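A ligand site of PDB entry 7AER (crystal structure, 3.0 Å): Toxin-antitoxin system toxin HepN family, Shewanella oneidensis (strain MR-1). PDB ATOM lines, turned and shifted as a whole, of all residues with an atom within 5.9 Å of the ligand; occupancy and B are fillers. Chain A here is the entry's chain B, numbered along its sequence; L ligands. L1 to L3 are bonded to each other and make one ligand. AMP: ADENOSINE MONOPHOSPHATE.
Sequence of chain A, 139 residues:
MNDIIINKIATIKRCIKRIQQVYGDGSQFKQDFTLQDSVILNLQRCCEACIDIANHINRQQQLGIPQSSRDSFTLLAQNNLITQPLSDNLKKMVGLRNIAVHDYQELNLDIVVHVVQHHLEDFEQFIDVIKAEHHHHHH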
ATOM      1  N   ARG A  70      -0.619   7.224 -10.799  1.00  0.00           N
ATOM      2  CA  ARG A  70      -0.742   8.624 -10.440  1.00  0.00           C
ATOM      3  C   ARG A  70      -1.671   8.820  -9.254  1.00  0.00           C
ATOM      4  O   ARG A  70      -1.428   9.698  -8.410  1.00  0.00           O
ATOM      5  CB  ARG A  70      -1.237   9.429 -11.637  1.00  0.00           C
ATOM      6  CG  ARG A  70      -0.228   9.576 -12.762  1.00  0.00           C
ATOM      7  CD  ARG A  70      -0.839  10.295 -13.945  1.00  0.00           C
ATOM      8  NE  ARG A  70       0.145  10.578 -14.975  1.00  0.00           N
ATOM      9  CZ  ARG A  70       0.510   9.705 -15.925  1.00  0.00           C
ATOM     10  NH1 ARG A  70      -0.031   8.498 -15.955  1.00  0.00           N
ATOM     11  NH2 ARG A  70       1.412  10.052 -16.826  1.00  0.00           N
ATOM     12  N   LYS A  91       3.778  12.917 -10.342  1.00  0.00           N
ATOM     13  CA  LYS A  91       2.881  12.358 -11.350  1.00  0.00           C
ATOM     14  C   LYS A  91       3.330  12.695 -12.762  1.00  0.00           C
ATOM     15  O   LYS A  91       3.167  11.878 -13.673  1.00  0.00           O
ATOM     16  CB  LYS A  91       1.452  12.826 -11.112  1.00  0.00           C
ATOM     17  CG  LYS A  91       0.762  12.133  -9.946  1.00  0.00           C
ATOM     18  CD  LYS A  91      -0.671  12.592  -9.785  1.00  0.00           C
ATOM     19  CE  LYS A  91      -0.740  14.041  -9.359  1.00  0.00           C
ATOM     20  NZ  LYS A  91      -2.142  14.470  -9.070  1.00  0.00           N
ATOM     21  N   LYS A  92       3.895  13.882 -12.970  1.00  0.00           N
ATOM     22  CA  LYS A  92       4.454  14.227 -14.273  1.00  0.00           C
ATOM     23  C   LYS A  92       5.758  13.509 -14.555  1.00  0.00           C
ATOM     24  O   LYS A  92       6.252  13.568 -15.694  1.00  0.00           O
ATOM     25  CB  LYS A  92       4.644  15.738 -14.380  1.00  0.00           C
ATOM     26  CG  LYS A  92       3.357  16.489 -14.680  1.00  0.00           C
ATOM     27  CD  LYS A  92       3.464  17.969 -14.343  1.00  0.00           C
ATOM     28  CE  LYS A  92       2.226  18.719 -14.787  1.00  0.00           C
ATOM     29  NZ  LYS A  92       2.262  20.157 -14.382  1.00  0.00           N
ATOM     30  N   MET A  93       6.329  12.826 -13.571  1.00  0.00           N
ATOM     31  CA  MET A  93       7.519  12.021 -13.771  1.00  0.00           C
ATOM     32  C   MET A  93       7.147  10.675 -14.374  1.00  0.00           C
ATOM     33  O   MET A  93       7.869  10.119 -15.199  1.00  0.00           O
ATOM     34  CB  MET A  93       8.277  11.832 -12.460  1.00  0.00           C
ATOM     35  CG  MET A  93       9.780  11.665 -12.618  1.00  0.00           C
ATOM     36  SD  MET A  93      10.588  13.175 -13.539  1.00  0.00           S
ATOM     37  CE  MET A  93       9.892  14.609 -12.420  1.00  0.00           C
ATOM     38  N   VAL A  94       5.993  10.152 -13.946  1.00  0.00           N
ATOM     39  CA  VAL A  94       5.478   8.905 -14.507  1.00  0.00           C
ATOM     40  C   VAL A  94       5.224   9.064 -16.003  1.00  0.00           C
ATOM     41  O   VAL A  94       5.500   8.156 -16.795  1.00  0.00           O
ATOM     42  CB  VAL A  94       4.204   8.464 -13.760  1.00  0.00           C
ATOM     43  CG1 VAL A  94       3.645   7.184 -14.365  1.00  0.00           C
ATOM     44  CG2 VAL A  94       4.489   8.277 -12.278  1.00  0.00           C
ATOM     45  N   GLY A  95       4.700  10.224 -16.406  1.00  0.00           N
ATOM     46  CA  GLY A  95       4.509  10.485 -17.821  1.00  0.00           C
ATOM     47  C   GLY A  95       5.813  10.445 -18.601  1.00  0.00           C
ATOM     48  O   GLY A  95       5.863   9.936 -19.719  1.00  0.00           O
ATOM     49  N   LEU A  96       6.888  10.983 -18.010  1.00  0.00           N
ATOM     50  CA  LEU A  96       8.194  10.894 -18.649  1.00  0.00           C
ATOM     51  C   LEU A  96       8.680   9.455 -18.710  1.00  0.00           C
ATOM     52  O   LEU A  96       9.301   9.046 -19.693  1.00  0.00           O
ATOM     53  CB  LEU A  96       9.200  11.773 -17.903  1.00  0.00           C
ATOM     54  CG  LEU A  96      10.621  11.780 -18.448  1.00  0.00           C
ATOM     55  CD1 LEU A  96      10.639  12.292 -19.883  1.00  0.00           C
ATOM     56  CD2 LEU A  96      11.522  12.623 -17.561  1.00  0.00           C
ATOM     57  N   ASN A  98       6.770   6.691 -18.915  1.00  0.00           N
ATOM     58  CA  ASN A  98       6.007   5.924 -19.893  1.00  0.00           C
ATOM     59  C   ASN A  98       6.365   6.310 -21.319  1.00  0.00           C
ATOM     60  O   ASN A  98       6.490   5.440 -22.191  1.00  0.00           O
ATOM     61  CB  ASN A  98       4.508   6.100 -19.658  1.00  0.00           C
ATOM     62  CG  ASN A  98       4.048   5.521 -18.334  1.00  0.00           C
ATOM     63  OD1 ASN A  98       4.675   4.609 -17.797  1.00  0.00           O
ATOM     64  ND2 ASN A  98       2.950   6.044 -17.809  1.00  0.00           N
ATOM     65  N   ILE A  99       6.539   7.605 -21.576  1.00  0.00           N
ATOM     66  CA  ILE A  99       6.916   8.059 -22.920  1.00  0.00           C
ATOM     67  C   ILE A  99       8.282   7.515 -23.310  1.00  0.00           C
ATOM     68  O   ILE A  99       8.532   7.194 -24.472  1.00  0.00           O
ATOM     69  CB  ILE A  99       6.855   9.602 -22.992  1.00  0.00           C
ATOM     70  CG1 ILE A  99       5.414  10.089 -22.884  1.00  0.00           C
ATOM     71  CG2 ILE A  99       7.463  10.113 -24.287  1.00  0.00           C
ATOM     72  CD1 ILE A  99       5.267  11.600 -23.040  1.00  0.00           C
ATOM     73  N   HIS A 102       7.823   2.792 -23.377  1.00  0.00           N
ATOM     74  CA  HIS A 102       7.082   2.436 -24.594  1.00  0.00           C
ATOM     75  C   HIS A 102       6.541   3.723 -25.193  1.00  0.00           C
ATOM     76  O   HIS A 102       5.587   4.316 -24.657  1.00  0.00           O
ATOM     77  CB  HIS A 102       5.972   1.438 -24.293  1.00  0.00           C
ATOM     78  CG  HIS A 102       5.296   1.644 -22.984  1.00  0.00           C
ATOM     79  ND1 HIS A 102       4.743   2.853 -22.596  1.00  0.00           N
ATOM     80  CD2 HIS A 102       5.086   0.787 -21.952  1.00  0.00           C
ATOM     81  CE1 HIS A 102       4.217   2.731 -21.390  1.00  0.00           C
ATOM     82  NE2 HIS A 102       4.412   1.485 -20.972  1.00  0.00           N
ATOM     83  N   TYR A 104       4.566   6.147 -26.999  1.00  0.00           N
ATOM     84  CA  TYR A 104       3.398   6.603 -27.718  1.00  0.00           C
ATOM     85  C   TYR A 104       3.500   8.085 -28.075  1.00  0.00           C
ATOM     86  O   TYR A 104       2.490   8.733 -28.340  1.00  0.00           O
ATOM     87  CB  TYR A 104       2.126   6.342 -26.908  1.00  0.00           C
ATOM     88  CG  TYR A 104       2.141   6.879 -25.495  1.00  0.00           C
ATOM     89  CD1 TYR A 104       1.712   8.171 -25.216  1.00  0.00           C
ATOM     90  CD2 TYR A 104       2.575   6.086 -24.435  1.00  0.00           C
ATOM     91  CE1 TYR A 104       1.728   8.665 -23.926  1.00  0.00           C
ATOM     92  CE2 TYR A 104       2.582   6.572 -23.136  1.00  0.00           C
ATOM     93  CZ  TYR A 104       2.157   7.863 -22.888  1.00  0.00           C
ATOM     94  OH  TYR A 104       2.161   8.352 -21.602  1.00  0.00           O
ATOM     95  N   GLN A 105       4.729   8.619 -28.102  1.00  0.00           N
ATOM     96  CA  GLN A 105       4.995  10.033 -28.290  1.00  0.00           C
ATOM     97  C   GLN A 105       6.510  10.199 -28.412  1.00  0.00           C
ATOM     98  O   GLN A 105       7.258   9.571 -27.664  1.00  0.00           O
ATOM     99  CB  GLN A 105       4.432  10.839 -27.122  1.00  0.00           C
ATOM    100  CG  GLN A 105       4.184  12.315 -27.411  1.00  0.00           C
ATOM    101  CD  GLN A 105       3.364  12.988 -26.320  1.00  0.00           C
ATOM    102  OE1 GLN A 105       2.709  12.316 -25.517  1.00  0.00           O
ATOM    103  NE2 GLN A 105       3.409  14.313 -26.295  1.00  0.00           N
ATOM    104  N   GLU A 106       6.987  11.024 -29.340  1.00  0.00           N
ATOM    105  CA  GLU A 106       8.426  11.096 -29.584  1.00  0.00           C
ATOM    106  C   GLU A 106       9.137  11.719 -28.390  1.00  0.00           C
ATOM    107  O   GLU A 106       8.756  12.800 -27.917  1.00  0.00           O
ATOM    108  CB  GLU A 106       8.723  11.887 -30.853  1.00  0.00           C
ATOM    109  CG  GLU A 106      10.209  11.970 -31.178  1.00  0.00           C
ATOM    110  CD  GLU A 106      10.472  12.294 -32.630  1.00  0.00           C
ATOM    111  OE1 GLU A 106       9.488  12.322 -33.408  1.00  0.00           O
ATOM    112  OE2 GLU A 106      11.640  12.525 -33.005  1.00  0.00           O
ATOM    113  N   LEU A 107      10.155  11.029 -27.893  1.00  0.00           N
ATOM    114  CA  LEU A 107      10.860  11.450 -26.682  1.00  0.00           C
ATOM    115  C   LEU A 107      11.615  12.751 -26.946  1.00  0.00           C
ATOM    116  O   LEU A 107      12.506  12.797 -27.801  1.00  0.00           O
ATOM    117  CB  LEU A 107      11.811  10.354 -26.218  1.00  0.00           C
ATOM    118  CG  LEU A 107      12.479  10.531 -24.852  1.00  0.00           C
ATOM    119  CD1 LEU A 107      11.445  10.490 -23.737  1.00  0.00           C
ATOM    120  CD2 LEU A 107      13.545   9.469 -24.623  1.00  0.00           C
ATOM    121  N   ASN A 108      11.265  13.789 -26.188  1.00  0.00           N
ATOM    122  CA  ASN A 108      11.984  15.061 -26.241  1.00  0.00           C
ATOM    123  C   ASN A 108      13.165  14.970 -25.283  1.00  0.00           C
ATOM    124  O   ASN A 108      12.978  14.983 -24.056  1.00  0.00           O
ATOM    125  CB  ASN A 108      11.066  16.218 -25.881  1.00  0.00           C
ATOM    126  CG  ASN A 108      11.672  17.577 -26.206  1.00  0.00           C
ATOM    127  OD1 ASN A 108      12.892  17.719 -26.289  1.00  0.00           O
ATOM    128  ND2 ASN A 108      10.812  18.573 -26.371  1.00  0.00           N
ATOM    129  N   LEU A 109      14.379  14.872 -25.826  1.00  0.00           N
ATOM    130  CA  LEU A 109      15.557  14.682 -24.991  1.00  0.00           C
ATOM    131  C   LEU A 109      15.854  15.917 -24.143  1.00  0.00           C
ATOM    132  O   LEU A 109      16.442  15.789 -23.067  1.00  0.00           O
ATOM    133  CB  LEU A 109      16.767  14.319 -25.855  1.00  0.00           C
ATOM    134  CG  LEU A 109      17.814  13.441 -25.176  1.00  0.00           C
ATOM    135  CD1 LEU A 109      17.219  12.098 -24.784  1.00  0.00           C
ATOM    136  CD2 LEU A 109      19.010  13.257 -26.092  1.00  0.00           C
ATOM    137  N   ASP A 110      15.453  17.103 -24.611  1.00  0.00           N
ATOM    138  CA  ASP A 110      15.628  18.313 -23.818  1.00  0.00           C
ATOM    139  C   ASP A 110      14.833  18.277 -22.531  1.00  0.00           C
ATOM    140  O   ASP A 110      15.158  19.008 -21.591  1.00  0.00           O
ATOM    141  CB  ASP A 110      15.232  19.537 -24.643  1.00  0.00           C
ATOM    142  CG  ASP A 110      16.343  20.000 -25.560  1.00  0.00           C
ATOM    143  OD1 ASP A 110      17.485  19.521 -25.395  1.00  0.00           O
ATOM    144  OD2 ASP A 110      16.073  20.850 -26.444  1.00  0.00           O
ATOM    145  N   ILE A 111      13.797  17.436 -22.451  1.00  0.00           N
ATOM    146  CA  ILE A 111      13.069  17.262 -21.197  1.00  0.00           C
ATOM    147  C   ILE A 111      13.863  16.391 -20.238  1.00  0.00           C
ATOM    148  O   ILE A 111      13.940  16.683 -19.036  1.00  0.00           O
ATOM    149  CB  ILE A 111      11.672  16.676 -21.480  1.00  0.00           C
ATOM    150  CG1 ILE A 111      10.858  17.636 -22.355  1.00  0.00           C
ATOM    151  CG2 ILE A 111      10.941  16.389 -20.170  1.00  0.00           C
ATOM    152  CD1 ILE A 111       9.470  17.137 -22.685  1.00  0.00           C
ATOM    153  N   VAL A 112      14.476  15.321 -20.739  1.00  0.00           N
ATOM    154  CA  VAL A 112      15.275  14.448 -19.888  1.00  0.00           C
ATOM    155  C   VAL A 112      16.494  15.194 -19.358  1.00  0.00           C
ATOM    156  O   VAL A 112      16.886  15.034 -18.201  1.00  0.00           O
ATOM    157  CB  VAL A 112      15.673  13.169 -20.654  1.00  0.00           C
ATOM    158  CG1 VAL A 112      16.264  12.146 -19.703  1.00  0.00           C
ATOM    159  CG2 VAL A 112      14.469  12.600 -21.390  1.00  0.00           C
ATOM    160  N   HIS A 114      16.613  18.402 -18.893  1.00  0.00           N
ATOM    161  CA  HIS A 114      16.095  19.368 -17.936  1.00  0.00           C
ATOM    162  C   HIS A 114      15.774  18.714 -16.595  1.00  0.00           C
ATOM    163  O   HIS A 114      15.976  19.327 -15.539  1.00  0.00           O
ATOM    164  CB  HIS A 114      14.867  20.070 -18.521  1.00  0.00           C
ATOM    165  CG  HIS A 114      14.311  21.160 -17.649  1.00  0.00           C
ATOM    166  ND1 HIS A 114      14.711  22.468 -17.773  1.00  0.00           N
ATOM    167  CD2 HIS A 114      13.405  21.131 -16.649  1.00  0.00           C
ATOM    168  CE1 HIS A 114      14.061  23.211 -16.891  1.00  0.00           C
ATOM    169  NE2 HIS A 114      13.272  22.420 -16.194  1.00  0.00           N
ATOM    170  N   VAL A 115      15.277  17.483 -16.614  1.00  0.00           N
ATOM    171  CA  VAL A 115      14.837  16.827 -15.386  1.00  0.00           C
ATOM    172  C   VAL A 115      16.037  16.465 -14.508  1.00  0.00           C
ATOM    173  O   VAL A 115      15.962  16.554 -13.273  1.00  0.00           O
ATOM    174  CB  VAL A 115      13.974  15.592 -15.717  1.00  0.00           C
ATOM    175  CG1 VAL A 115      13.843  14.679 -14.511  1.00  0.00           C
ATOM    176  CG2 VAL A 115      12.602  16.028 -16.208  1.00  0.00           C
ATOM    177  N   HIS A 119      15.036  18.599 -11.426  1.00  0.00           N
ATOM    178  CA  HIS A 119      13.944  17.769 -10.911  1.00  0.00           C
ATOM    179  C   HIS A 119      14.374  16.596 -10.050  1.00  0.00           C
ATOM    180  O   HIS A 119      13.505  15.940  -9.468  1.00  0.00           O
ATOM    181  CB  HIS A 119      13.075  17.255 -12.071  1.00  0.00           C
ATOM    182  CG  HIS A 119      12.028  18.219 -12.514  1.00  0.00           C
ATOM    183  ND1 HIS A 119      11.258  18.936 -11.620  1.00  0.00           N
ATOM    184  CD2 HIS A 119      11.617  18.595 -13.744  1.00  0.00           C
ATOM    185  CE1 HIS A 119      10.412  19.706 -12.294  1.00  0.00           C
ATOM    186  NE2 HIS A 119      10.610  19.518 -13.581  1.00  0.00           N
HETATM  187  P   AMP L   1       1.380   8.613 -20.248  1.00  0.00           P
HETATM  188  O1P AMP L   1      -0.068   8.929 -20.547  1.00  0.00           O
HETATM  189  O2P AMP L   1       1.717   7.566 -19.219  1.00  0.00           O
HETATM  190  O5' AMP L   1       2.115   9.972 -19.829  1.00  0.00           O
HETATM  191  C5' AMP L   1       2.398  10.969 -20.804  1.00  0.00           C
HETATM  192  C4' AMP L   1       1.689  12.264 -20.486  1.00  0.00           C
HETATM  193  O4' AMP L   1       1.170  12.799 -21.727  1.00  0.00           O
HETATM  194  C3' AMP L   1       0.506  12.100 -19.527  1.00  0.00           C
HETATM  195  O3' AMP L   1       0.633  12.933 -18.360  1.00  0.00           O
HETATM  196  C2' AMP L   1      -0.738  12.451 -20.355  1.00  0.00           C
HETATM  197  O2' AMP L   1      -1.685  13.243 -19.669  1.00  0.00           O
HETATM  198  C1' AMP L   1      -0.180  13.168 -21.580  1.00  0.00           C
HETATM  199  N9  AMP L   1      -0.864  12.817 -22.829  1.00  0.00           N
HETATM  200  C8  AMP L   1      -1.819  11.867 -22.948  1.00  0.00           C
HETATM  201  N7  AMP L   1      -2.253  11.767 -24.223  1.00  0.00           N
HETATM  202  C5  AMP L   1      -1.572  12.673 -24.953  1.00  0.00           C
HETATM  203  C6  AMP L   1      -1.540  13.086 -26.374  1.00  0.00           C
HETATM  204  N6  AMP L   1      -2.350  12.502 -27.287  1.00  0.00           N
HETATM  205  N1  AMP L   1      -0.679  14.060 -26.726  1.00  0.00           N
HETATM  206  C2  AMP L   1       0.126  14.647 -25.827  1.00  0.00           C
HETATM  207  N3  AMP L   1       0.155  14.328 -24.521  1.00  0.00           N
HETATM  208  C4  AMP L   1      -0.661  13.362 -24.031  1.00  0.00           C
HETATM  209  P   AMP L   2       1.209  14.429 -18.384  1.00  0.00           P
HETATM  210  O1P AMP L   2       0.801  15.200 -19.616  1.00  0.00           O
HETATM  211  O2P AMP L   2       0.849  15.021 -17.036  1.00  0.00           O
HETATM  212  O5' AMP L   2       2.787  14.276 -18.383  1.00  0.00           O
HETATM  213  C5' AMP L   2       3.622  15.419 -18.506  1.00  0.00           C
HETATM  214  C4' AMP L   2       5.082  15.055 -18.500  1.00  0.00           C
HETATM  215  O4' AMP L   2       5.347  14.079 -19.535  1.00  0.00           O
HETATM  216  C3' AMP L   2       6.054  16.185 -18.806  1.00  0.00           C
HETATM  217  O3' AMP L   2       6.299  17.035 -17.704  1.00  0.00           O
HETATM  218  C2' AMP L   2       7.281  15.444 -19.301  1.00  0.00           C
HETATM  219  O2' AMP L   2       8.039  14.941 -18.200  1.00  0.00           O
HETATM  220  C1' AMP L   2       6.655  14.259 -20.040  1.00  0.00           C
HETATM  221  N9  AMP L   2       6.579  14.492 -21.490  1.00  0.00           N
HETATM  222  C8  AMP L   2       5.536  15.027 -22.152  1.00  0.00           C
HETATM  223  N7  AMP L   2       5.789  15.105 -23.481  1.00  0.00           N
HETATM  224  C5  AMP L   2       7.025  14.605 -23.692  1.00  0.00           C
HETATM  225  C6  AMP L   2       7.913  14.397 -24.860  1.00  0.00           C
HETATM  226  N6  AMP L   2       7.519  14.740 -26.110  1.00  0.00           N
HETATM  227  N1  AMP L   2       9.116  13.839 -24.632  1.00  0.00           N
HETATM  228  C2  AMP L   2       9.522  13.500 -23.401  1.00  0.00           C
HETATM  229  N3  AMP L   2       8.781  13.665 -22.296  1.00  0.00           N
HETATM  230  C4  AMP L   2       7.539  14.207 -22.371  1.00  0.00           C
HETATM  231  P   AMP L   3       6.013  18.597 -17.827  1.00  0.00           P
HETATM  232  O1P AMP L   3       6.147  18.979 -19.288  1.00  0.00           O
HETATM  233  O2P AMP L   3       4.729  18.900 -17.102  1.00  0.00           O
HETATM  234  O5' AMP L   3       7.199  19.288 -17.025  1.00  0.00           O
HETATM  235  C5' AMP L   3       8.481  18.679 -16.931  1.00  0.00           C
HETATM  236  C4' AMP L   3       9.596  19.691 -16.837  1.00  0.00           C
HETATM  237  O4' AMP L   3      10.250  19.814 -18.123  1.00  0.00           O
HETATM  238  C3' AMP L   3       9.176  21.102 -16.425  1.00  0.00           C
HETATM  239  O3' AMP L   3      10.134  21.641 -15.509  1.00  0.00           O
HETATM  240  C2' AMP L   3       9.224  21.879 -17.737  1.00  0.00           C
HETATM  241  O2' AMP L   3       9.491  23.265 -17.590  1.00  0.00           O
HETATM  242  C1' AMP L   3      10.331  21.172 -18.496  1.00  0.00           C
HETATM  243  N9  AMP L   3      10.186  21.250 -19.953  1.00  0.00           N
HETATM  244  C8  AMP L   3       9.015  21.172 -20.599  1.00  0.00           C
HETATM  245  N7  AMP L   3       9.172  21.291 -21.943  1.00  0.00           N
HETATM  246  C5  AMP L   3      10.490  21.450 -22.176  1.00  0.00           C
HETATM  247  C6  AMP L   3      11.339  21.626 -23.371  1.00  0.00           C
HETATM  248  N6  AMP L   3      10.796  21.652 -24.617  1.00  0.00           N
HETATM  249  N1  AMP L   3      12.669  21.762 -23.189  1.00  0.00           N
HETATM  250  C2  AMP L   3      13.216  21.733 -21.952  1.00  0.00           C
HETATM  251  N3  AMP L   3      12.501  21.577 -20.827  1.00  0.00           N
HETATM  252  C4  AMP L   3      11.151  21.428 -20.861  1.00  0.00           C
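ND2 of Asn 98 sits close to O of Val 94 (3.5 Å).
O of Asn 98 sits at hydrogen-bond distance from ND1 of His 102 (3.1 Å).
OD1 of Asn 108 is in hydrogen-bond range of N of Asp 110 (3.1 Å).
The side-chain hydroxyl (OH) of Tyr 104 is covalently linked to a phosphorus (P) of AMP L1, 1.6 Å away.
The side-chain amide nitrogen (ND2) of Asn 98 sits at hydrogen-bond distance from an oxygen (O2P) of AMP L1.
The backbone NH (N) of Asn 108 is in hydrogen-bond range of a nitrogen (N1) of AMP L2 (2.7 Å).
NE2 of His 119 lies within hydrogen-bond range of O3' of AMP L3 (2.9 Å).
A nitrogen (N6) of AMP L2 sits at hydrogen-bond distance from the backbone carbonyl oxygen (O) of Glu 106, at 2.9 Å.
An oxygen (O2P) of AMP L1 is in salt-bridge range of the guanidinium group of Arg 70 (3.5 Å).
The backbone carbonyl oxygen of Lys 92 lies within hydrogen-bond range of an oxygen (O2') of AMP L2.
The side-chain amino group (NZ) of Lys 92 is in salt-bridge range of an oxygen (O2P) of AMP L3 (3.9 Å).
O3' of AMP L3 is in hydrogen-bond range of NE2 of His 114 (3.3 Å).
The side-chain amide oxygen of Gln 105 lies close to a nitrogen (N3) of AMP L1, at 3.4 Å.
Gly 95 touches the ligand.
Leu 96 touches the ligand.
CD1 of Ile 99 touches C4 of AMP L2 (3.5 Å).
Leu 107 touches the ligand.
O of Asp 110 touches C2 of AMP L3 (3.4 Å).
Ile 111 touches the ligand.
Of the 22 residues printed, 15 come within 4 Å of the ligand.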
